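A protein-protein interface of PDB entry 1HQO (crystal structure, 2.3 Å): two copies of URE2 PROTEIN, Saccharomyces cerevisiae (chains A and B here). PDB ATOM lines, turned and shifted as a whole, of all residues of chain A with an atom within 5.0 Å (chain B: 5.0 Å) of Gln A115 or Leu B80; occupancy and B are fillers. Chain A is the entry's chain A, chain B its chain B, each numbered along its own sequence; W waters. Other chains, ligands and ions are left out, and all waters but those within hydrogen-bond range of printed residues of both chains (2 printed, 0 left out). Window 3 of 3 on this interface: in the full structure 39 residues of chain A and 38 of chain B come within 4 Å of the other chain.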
ATOM      1  N   ALA A 111      17.493   1.391 -11.124  1.00  0.00           N
ATOM      2  CA  ALA A 111      18.539   0.501 -10.619  1.00  0.00           C
ATOM      3  C   ALA A 111      18.588  -0.792 -11.469  1.00  0.00           C
ATOM      4  O   ALA A 111      19.626  -1.455 -11.584  1.00  0.00           O
ATOM      5  CB  ALA A 111      18.286   0.170  -9.154  1.00  0.00           C
ATOM      6  N   ASP A 112      17.455  -1.143 -12.066  1.00  0.00           N
ATOM      7  CA  ASP A 112      17.363  -2.329 -12.908  1.00  0.00           C
ATOM      8  C   ASP A 112      18.062  -2.038 -14.236  1.00  0.00           C
ATOM      9  O   ASP A 112      18.816  -2.859 -14.746  1.00  0.00           O
ATOM     10  CB  ASP A 112      15.887  -2.693 -13.150  1.00  0.00           C
ATOM     11  CG  ASP A 112      15.408  -3.850 -12.271  1.00  0.00           C
ATOM     12  OD1 ASP A 112      16.194  -4.347 -11.424  1.00  0.00           O
ATOM     13  OD2 ASP A 112      14.235  -4.269 -12.437  1.00  0.00           O
ATOM     14  N   GLN A 113      17.818  -0.858 -14.786  1.00  0.00           N
ATOM     15  CA  GLN A 113      18.421  -0.490 -16.050  1.00  0.00           C
ATOM     16  C   GLN A 113      19.927  -0.413 -15.937  1.00  0.00           C
ATOM     17  O   GLN A 113      20.629  -0.866 -16.828  1.00  0.00           O
ATOM     18  CB  GLN A 113      17.903   0.856 -16.517  1.00  0.00           C
ATOM     19  CG  GLN A 113      16.411   0.922 -16.671  1.00  0.00           C
ATOM     20  CD  GLN A 113      15.942   2.332 -17.018  1.00  0.00           C
ATOM     21  OE1 GLN A 113      16.511   3.314 -16.538  1.00  0.00           O
ATOM     22  NE2 GLN A 113      14.897   2.438 -17.842  1.00  0.00           N
ATOM     23  N   SER A 114      20.424   0.157 -14.845  1.00  0.00           N
ATOM     24  CA  SER A 114      21.858   0.289 -14.671  1.00  0.00           C
ATOM     25  C   SER A 114      22.508  -1.083 -14.723  1.00  0.00           C
ATOM     26  O   SER A 114      23.665  -1.223 -15.120  1.00  0.00           O
ATOM     27  CB  SER A 114      22.182   0.968 -13.340  1.00  0.00           C
ATOM     28  OG  SER A 114      22.570   0.023 -12.358  1.00  0.00           O
ATOM     29  N   GLN A 115      21.752  -2.103 -14.328  1.00  0.00           N
ATOM     30  CA  GLN A 115      22.266  -3.468 -14.317  1.00  0.00           C
ATOM     31  C   GLN A 115      22.217  -4.084 -15.699  1.00  0.00           C
ATOM     32  O   GLN A 115      23.106  -4.854 -16.054  1.00  0.00           O
ATOM     33  CB  GLN A 115      21.487  -4.336 -13.316  1.00  0.00           C
ATOM     34  CG  GLN A 115      21.704  -3.930 -11.856  1.00  0.00           C
ATOM     35  CD  GLN A 115      23.175  -3.926 -11.446  1.00  0.00           C
ATOM     36  OE1 GLN A 115      23.824  -4.981 -11.360  1.00  0.00           O
ATOM     37  NE2 GLN A 115      23.709  -2.729 -11.196  1.00  0.00           N
ATOM     38  N   ILE A 116      21.175  -3.749 -16.463  1.00  0.00           N
ATOM     39  CA  ILE A 116      21.011  -4.242 -17.826  1.00  0.00           C
ATOM     40  C   ILE A 116      22.142  -3.649 -18.664  1.00  0.00           C
ATOM     41  O   ILE A 116      22.754  -4.338 -19.477  1.00  0.00           O
ATOM     42  CB  ILE A 116      19.663  -3.803 -18.416  1.00  0.00           C
ATOM     43  CG1 ILE A 116      18.530  -4.561 -17.717  1.00  0.00           C
ATOM     44  CG2 ILE A 116      19.646  -4.028 -19.918  1.00  0.00           C
ATOM     45  CD1 ILE A 116      17.134  -4.020 -18.015  1.00  0.00           C
ATOM     46  N   ASN A 117      22.423  -2.368 -18.442  1.00  0.00           N
ATOM     47  CA  ASN A 117      23.485  -1.688 -19.164  1.00  0.00           C
ATOM     48  C   ASN A 117      24.833  -2.321 -18.805  1.00  0.00           C
ATOM     49  O   ASN A 117      25.661  -2.558 -19.676  1.00  0.00           O
ATOM     50  CB  ASN A 117      23.496  -0.189 -18.825  1.00  0.00           C
ATOM     51  CG  ASN A 117      22.235   0.546 -19.309  1.00  0.00           C
ATOM     52  OD1 ASN A 117      21.510   0.066 -20.183  1.00  0.00           O
ATOM     53  ND2 ASN A 117      21.990   1.730 -18.745  1.00  0.00           N
ATOM     54  N   ALA A 118      25.046  -2.605 -17.524  1.00  0.00           N
ATOM     55  CA  ALA A 118      26.288  -3.225 -17.090  1.00  0.00           C
ATOM     56  C   ALA A 118      26.558  -4.498 -17.875  1.00  0.00           C
ATOM     57  O   ALA A 118      27.665  -4.700 -18.335  1.00  0.00           O
ATOM     58  CB  ALA A 118      26.232  -3.545 -15.603  1.00  0.00           C
ATOM     59  N   TRP A 119      25.547  -5.358 -18.015  1.00  0.00           N
ATOM     60  CA  TRP A 119      25.699  -6.610 -18.746  1.00  0.00           C
ATOM     61  C   TRP A 119      25.858  -6.352 -20.231  1.00  0.00           C
ATOM     62  O   TRP A 119      26.568  -7.090 -20.909  1.00  0.00           O
ATOM     63  CB  TRP A 119      24.503  -7.568 -18.515  1.00  0.00           C
ATOM     64  CG  TRP A 119      24.503  -8.218 -17.148  1.00  0.00           C
ATOM     65  CD1 TRP A 119      23.739  -7.864 -16.078  1.00  0.00           C
ATOM     66  CD2 TRP A 119      25.426  -9.203 -16.664  1.00  0.00           C
ATOM     67  NE1 TRP A 119      24.139  -8.544 -14.955  1.00  0.00           N
ATOM     68  CE2 TRP A 119      25.175  -9.372 -15.283  1.00  0.00           C
ATOM     69  CE3 TRP A 119      26.454  -9.946 -17.259  1.00  0.00           C
ATOM     70  CZ2 TRP A 119      25.903 -10.252 -14.489  1.00  0.00           C
ATOM     71  CZ3 TRP A 119      27.177 -10.820 -16.476  1.00  0.00           C
ATOM     72  CH2 TRP A 119      26.900 -10.964 -15.095  1.00  0.00           C
ATOM     73  N   VAL A 206      18.813 -10.158 -15.260  1.00  0.00           N
ATOM     74  CA  VAL A 206      18.281  -9.027 -14.523  1.00  0.00           C
ATOM     75  C   VAL A 206      16.760  -9.067 -14.386  1.00  0.00           C
ATOM     76  O   VAL A 206      16.043  -9.390 -15.339  1.00  0.00           O
ATOM     77  CB  VAL A 206      18.704  -7.659 -15.179  1.00  0.00           C
ATOM     78  CG1 VAL A 206      18.318  -6.511 -14.264  1.00  0.00           C
ATOM     79  CG2 VAL A 206      20.212  -7.618 -15.456  1.00  0.00           C
ATOM     80  N   LEU B  72      31.224   1.490  -9.121  1.00  0.00           N
ATOM     81  CA  LEU B  72      30.668   2.638  -8.408  1.00  0.00           C
ATOM     82  C   LEU B  72      29.481   2.258  -7.553  1.00  0.00           C
ATOM     83  O   LEU B  72      28.516   1.639  -8.027  1.00  0.00           O
ATOM     84  CB  LEU B  72      30.186   3.722  -9.382  1.00  0.00           C
ATOM     85  CG  LEU B  72      29.806   5.052  -8.735  1.00  0.00           C
ATOM     86  CD1 LEU B  72      31.083   5.804  -8.479  1.00  0.00           C
ATOM     87  CD2 LEU B  72      28.896   5.884  -9.615  1.00  0.00           C
ATOM     88  N   ILE B  73      29.538   2.641  -6.286  1.00  0.00           N
ATOM     89  CA  ILE B  73      28.422   2.361  -5.412  1.00  0.00           C
ATOM     90  C   ILE B  73      27.642   3.643  -5.212  1.00  0.00           C
ATOM     91  O   ILE B  73      28.193   4.673  -4.792  1.00  0.00           O
ATOM     92  CB  ILE B  73      28.886   1.814  -4.069  1.00  0.00           C
ATOM     93  CG1 ILE B  73      29.534   0.457  -4.287  1.00  0.00           C
ATOM     94  CG2 ILE B  73      27.705   1.658  -3.132  1.00  0.00           C
ATOM     95  CD1 ILE B  73      30.958   0.459  -3.947  1.00  0.00           C
ATOM     96  N   ASP B  74      26.366   3.575  -5.570  1.00  0.00           N
ATOM     97  CA  ASP B  74      25.457   4.700  -5.428  1.00  0.00           C
ATOM     98  C   ASP B  74      24.725   4.499  -4.106  1.00  0.00           C
ATOM     99  O   ASP B  74      23.651   3.892  -4.049  1.00  0.00           O
ATOM    100  CB  ASP B  74      24.468   4.735  -6.594  1.00  0.00           C
ATOM    101  CG  ASP B  74      23.352   5.731  -6.383  1.00  0.00           C
ATOM    102  OD1 ASP B  74      23.462   6.577  -5.470  1.00  0.00           O
ATOM    103  OD2 ASP B  74      22.360   5.675  -7.139  1.00  0.00           O
ATOM    104  N   MET B  77      21.190   4.988  -3.290  1.00  0.00           N
ATOM    105  CA  MET B  77      20.311   3.941  -3.785  1.00  0.00           C
ATOM    106  C   MET B  77      20.573   2.549  -3.211  1.00  0.00           C
ATOM    107  O   MET B  77      20.714   1.569  -3.948  1.00  0.00           O
ATOM    108  CB  MET B  77      20.375   3.897  -5.319  1.00  0.00           C
ATOM    109  CG  MET B  77      19.677   5.074  -6.011  1.00  0.00           C
ATOM    110  SD  MET B  77      19.529   4.940  -7.974  1.00  0.00           S
ATOM    111  CE  MET B  77      17.890   3.899  -8.171  1.00  0.00           C
ATOM    112  N   ASP B  78      20.618   2.464  -1.886  1.00  0.00           N
ATOM    113  CA  ASP B  78      20.833   1.192  -1.199  1.00  0.00           C
ATOM    114  C   ASP B  78      22.092   0.510  -1.656  1.00  0.00           C
ATOM    115  O   ASP B  78      22.067  -0.681  -1.966  1.00  0.00           O
ATOM    116  CB  ASP B  78      19.671   0.219  -1.437  1.00  0.00           C
ATOM    117  CG  ASP B  78      18.320   0.816  -1.073  1.00  0.00           C
ATOM    118  OD1 ASP B  78      18.247   1.568  -0.066  1.00  0.00           O
ATOM    119  OD2 ASP B  78      17.325   0.518  -1.791  1.00  0.00           O
ATOM    120  N   ASN B  79      23.184   1.259  -1.707  1.00  0.00           N
ATOM    121  CA  ASN B  79      24.463   0.704  -2.134  1.00  0.00           C
ATOM    122  C   ASN B  79      24.454  -0.059  -3.466  1.00  0.00           C
ATOM    123  O   ASN B  79      25.166  -1.068  -3.612  1.00  0.00           O
ATOM    124  CB  ASN B  79      25.016  -0.199  -1.045  1.00  0.00           C
ATOM    125  CG  ASN B  79      25.223   0.537   0.242  1.00  0.00           C
ATOM    126  OD1 ASN B  79      25.864   1.600   0.272  1.00  0.00           O
ATOM    127  ND2 ASN B  79      24.678  -0.009   1.324  1.00  0.00           N
ATOM    128  N   LEU B  80      23.644   0.418  -4.418  1.00  0.00           N
ATOM    129  CA  LEU B  80      23.553  -0.166  -5.766  1.00  0.00           C
ATOM    130  C   LEU B  80      24.964  -0.128  -6.343  1.00  0.00           C
ATOM    131  O   LEU B  80      25.706   0.838  -6.121  1.00  0.00           O
ATOM    132  CB  LEU B  80      22.641   0.684  -6.659  1.00  0.00           C
ATOM    133  CG  LEU B  80      22.550   0.309  -8.142  1.00  0.00           C
ATOM    134  CD1 LEU B  80      22.011  -1.115  -8.268  1.00  0.00           C
ATOM    135  CD2 LEU B  80      21.630   1.283  -8.887  1.00  0.00           C
ATOM    136  N   SER B  81      25.352  -1.166  -7.070  1.00  0.00           N
ATOM    137  CA  SER B  81      26.682  -1.175  -7.640  1.00  0.00           C
ATOM    138  C   SER B  81      26.603  -1.248  -9.162  1.00  0.00           C
ATOM    139  O   SER B  81      25.951  -2.138  -9.704  1.00  0.00           O
ATOM    140  CB  SER B  81      27.458  -2.367  -7.090  1.00  0.00           C
ATOM    141  OG  SER B  81      28.785  -2.377  -7.573  1.00  0.00           O
ATOM    142  N   ILE B  82      27.216  -0.285  -9.850  1.00  0.00           N
ATOM    143  CA  ILE B  82      27.262  -0.316 -11.317  1.00  0.00           C
ATOM    144  C   ILE B  82      28.741  -0.597 -11.620  1.00  0.00           C
ATOM    145  O   ILE B  82      29.638   0.184 -11.278  1.00  0.00           O
ATOM    146  CB  ILE B  82      26.805   1.009 -11.975  1.00  0.00           C
ATOM    147  CG1 ILE B  82      25.456   1.462 -11.401  1.00  0.00           C
ATOM    148  CG2 ILE B  82      26.629   0.795 -13.466  1.00  0.00           C
ATOM    149  CD1 ILE B  82      25.602   2.397 -10.224  1.00  0.00           C
ATOM    150  N   TRP B  83      28.981  -1.728 -12.267  1.00  0.00           N
ATOM    151  CA  TRP B  83      30.338  -2.190 -12.524  1.00  0.00           C
ATOM    152  C   TRP B  83      30.978  -2.091 -13.916  1.00  0.00           C
ATOM    153  O   TRP B  83      31.994  -2.744 -14.154  1.00  0.00           O
ATOM    154  CB  TRP B  83      30.434  -3.635 -12.027  1.00  0.00           C
ATOM    155  CG  TRP B  83      29.233  -4.434 -12.439  1.00  0.00           C
ATOM    156  CD1 TRP B  83      27.965  -4.332 -11.930  1.00  0.00           C
ATOM    157  CD2 TRP B  83      29.160  -5.405 -13.498  1.00  0.00           C
ATOM    158  NE1 TRP B  83      27.104  -5.178 -12.607  1.00  0.00           N
ATOM    159  CE2 TRP B  83      27.811  -5.847 -13.573  1.00  0.00           C
ATOM    160  CE3 TRP B  83      30.097  -5.941 -14.389  1.00  0.00           C
ATOM    161  CZ2 TRP B  83      27.386  -6.799 -14.496  1.00  0.00           C
ATOM    162  CZ3 TRP B  83      29.670  -6.889 -15.305  1.00  0.00           C
ATOM    163  CH2 TRP B  83      28.325  -7.307 -15.350  1.00  0.00           C
ATOM    164  N   HIS B  91      24.384   5.827 -16.009  1.00  0.00           N
ATOM    165  CA  HIS B  91      23.661   5.903 -14.748  1.00  0.00           C
ATOM    166  C   HIS B  91      23.725   7.345 -14.262  1.00  0.00           C
ATOM    167  O   HIS B  91      22.708   8.012 -14.132  1.00  0.00           O
ATOM    168  CB  HIS B  91      24.287   4.969 -13.700  1.00  0.00           C
ATOM    169  CG  HIS B  91      23.528   4.910 -12.400  1.00  0.00           C
ATOM    170  ND1 HIS B  91      22.244   4.408 -12.302  1.00  0.00           N
ATOM    171  CD2 HIS B  91      23.881   5.285 -11.145  1.00  0.00           C
ATOM    172  CE1 HIS B  91      21.842   4.474 -11.045  1.00  0.00           C
ATOM    173  NE2 HIS B  91      22.816   5.004 -10.323  1.00  0.00           N
HETATM  174  O   HOH W   1      23.145   2.813 -16.644  1.00  0.00           O
HETATM  175  O   HOH W   2      20.751   3.536 -14.183  1.00  0.00           O
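The side-chain amide nitrogen (NE2) of Gln A115 sits at hydrogen-bond distance from the backbone carbonyl oxygen (O) of Ser B81, 2.8 Å away.
Of the 10 printed residues of chain A, 5 touch a printed residue of chain B.
Hydrophobic or aromatic side chains of chain A within 4 Å of the printed part of chain B: Ala A111, Ala A118 and Trp A119.
Along chain B the printed residues that touch a printed residue of chain A span positions 77 to 91.
Among the printed residues, 10 pairs touch across the chains.
O of Ala A111 sits at hydrogen-bond distance from OG of Ser A114.
The side-chain hydroxyl of Ser A114 is in hydrogen-bond range of the side-chain amide nitrogen of Gln A115 (3.2 Å).
The backbone carbonyl oxygen (O) of Leu B72 lies within hydrogen-bond range of the backbone NH (N) of Ile B82, at 3.0 Å.
N of Asp B74 sits at hydrogen-bond distance from O of Leu B80 (2.9 Å).
A ring nitrogen (NE2) of His B91 is in hydrogen-bond range of the side-chain carboxylate of Asp B74 (3.3 Å).
No position is printed for both chains.
Printed residues of chain B within 4 Å of Ser A114: Leu B80, Ile B82 and His B91.
Gln A115 touches just these residues of chain B: Leu B80, Ser B81 and Trp B83.
Of the printed residues of chain B, Trp A119 touches Trp B83 (3.5 Å).
Val A206 touches none of the printed residues of chain B.
Asp B78 touches none of the printed residues of chain A.
Of the printed residues of chain A, Leu B80 touches Ala A111, Ser A114 and Gln A115.
Of the printed residues of chain A, Ser B81 touches Gln A115.
Of the printed residues of chain A, Trp B83 touches Gln A115, Ala A118 and Trp A119.
Of the printed residues of chain A, His B91 touches Ser A114 (3.6 Å).
The nearest printed residue of chain A that does not touch Leu B80 is Asp A112 (5.8 Å).
Water W2 lies within hydrogen-bond range of ND1 of His B91 (2.6 Å) and N of Ser A114 (3.5 Å).
Water W1 lies within hydrogen-bond range of ND2 of Asn A117 (2.6 Å) and N of His B91 (3.3 Å).
Among the printed residues, pairs that only touch across the chains: Ser A114 with Ile B82 (3.4 Å), Ala A118 with Trp B83 (3.5 Å), Trp A119 with Trp B83 (3.5 Å), Gln A115 with Trp B83 (3.5 Å), Ala A111 with Leu B80 (3.5 Å), Ser A114 with His B91 (3.6 Å), Gln A115 with Leu B80 (3.7 Å), Ser A114 with Leu B80 (3.8 Å) and Ala A111 with Met B77 (3.9 Å).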
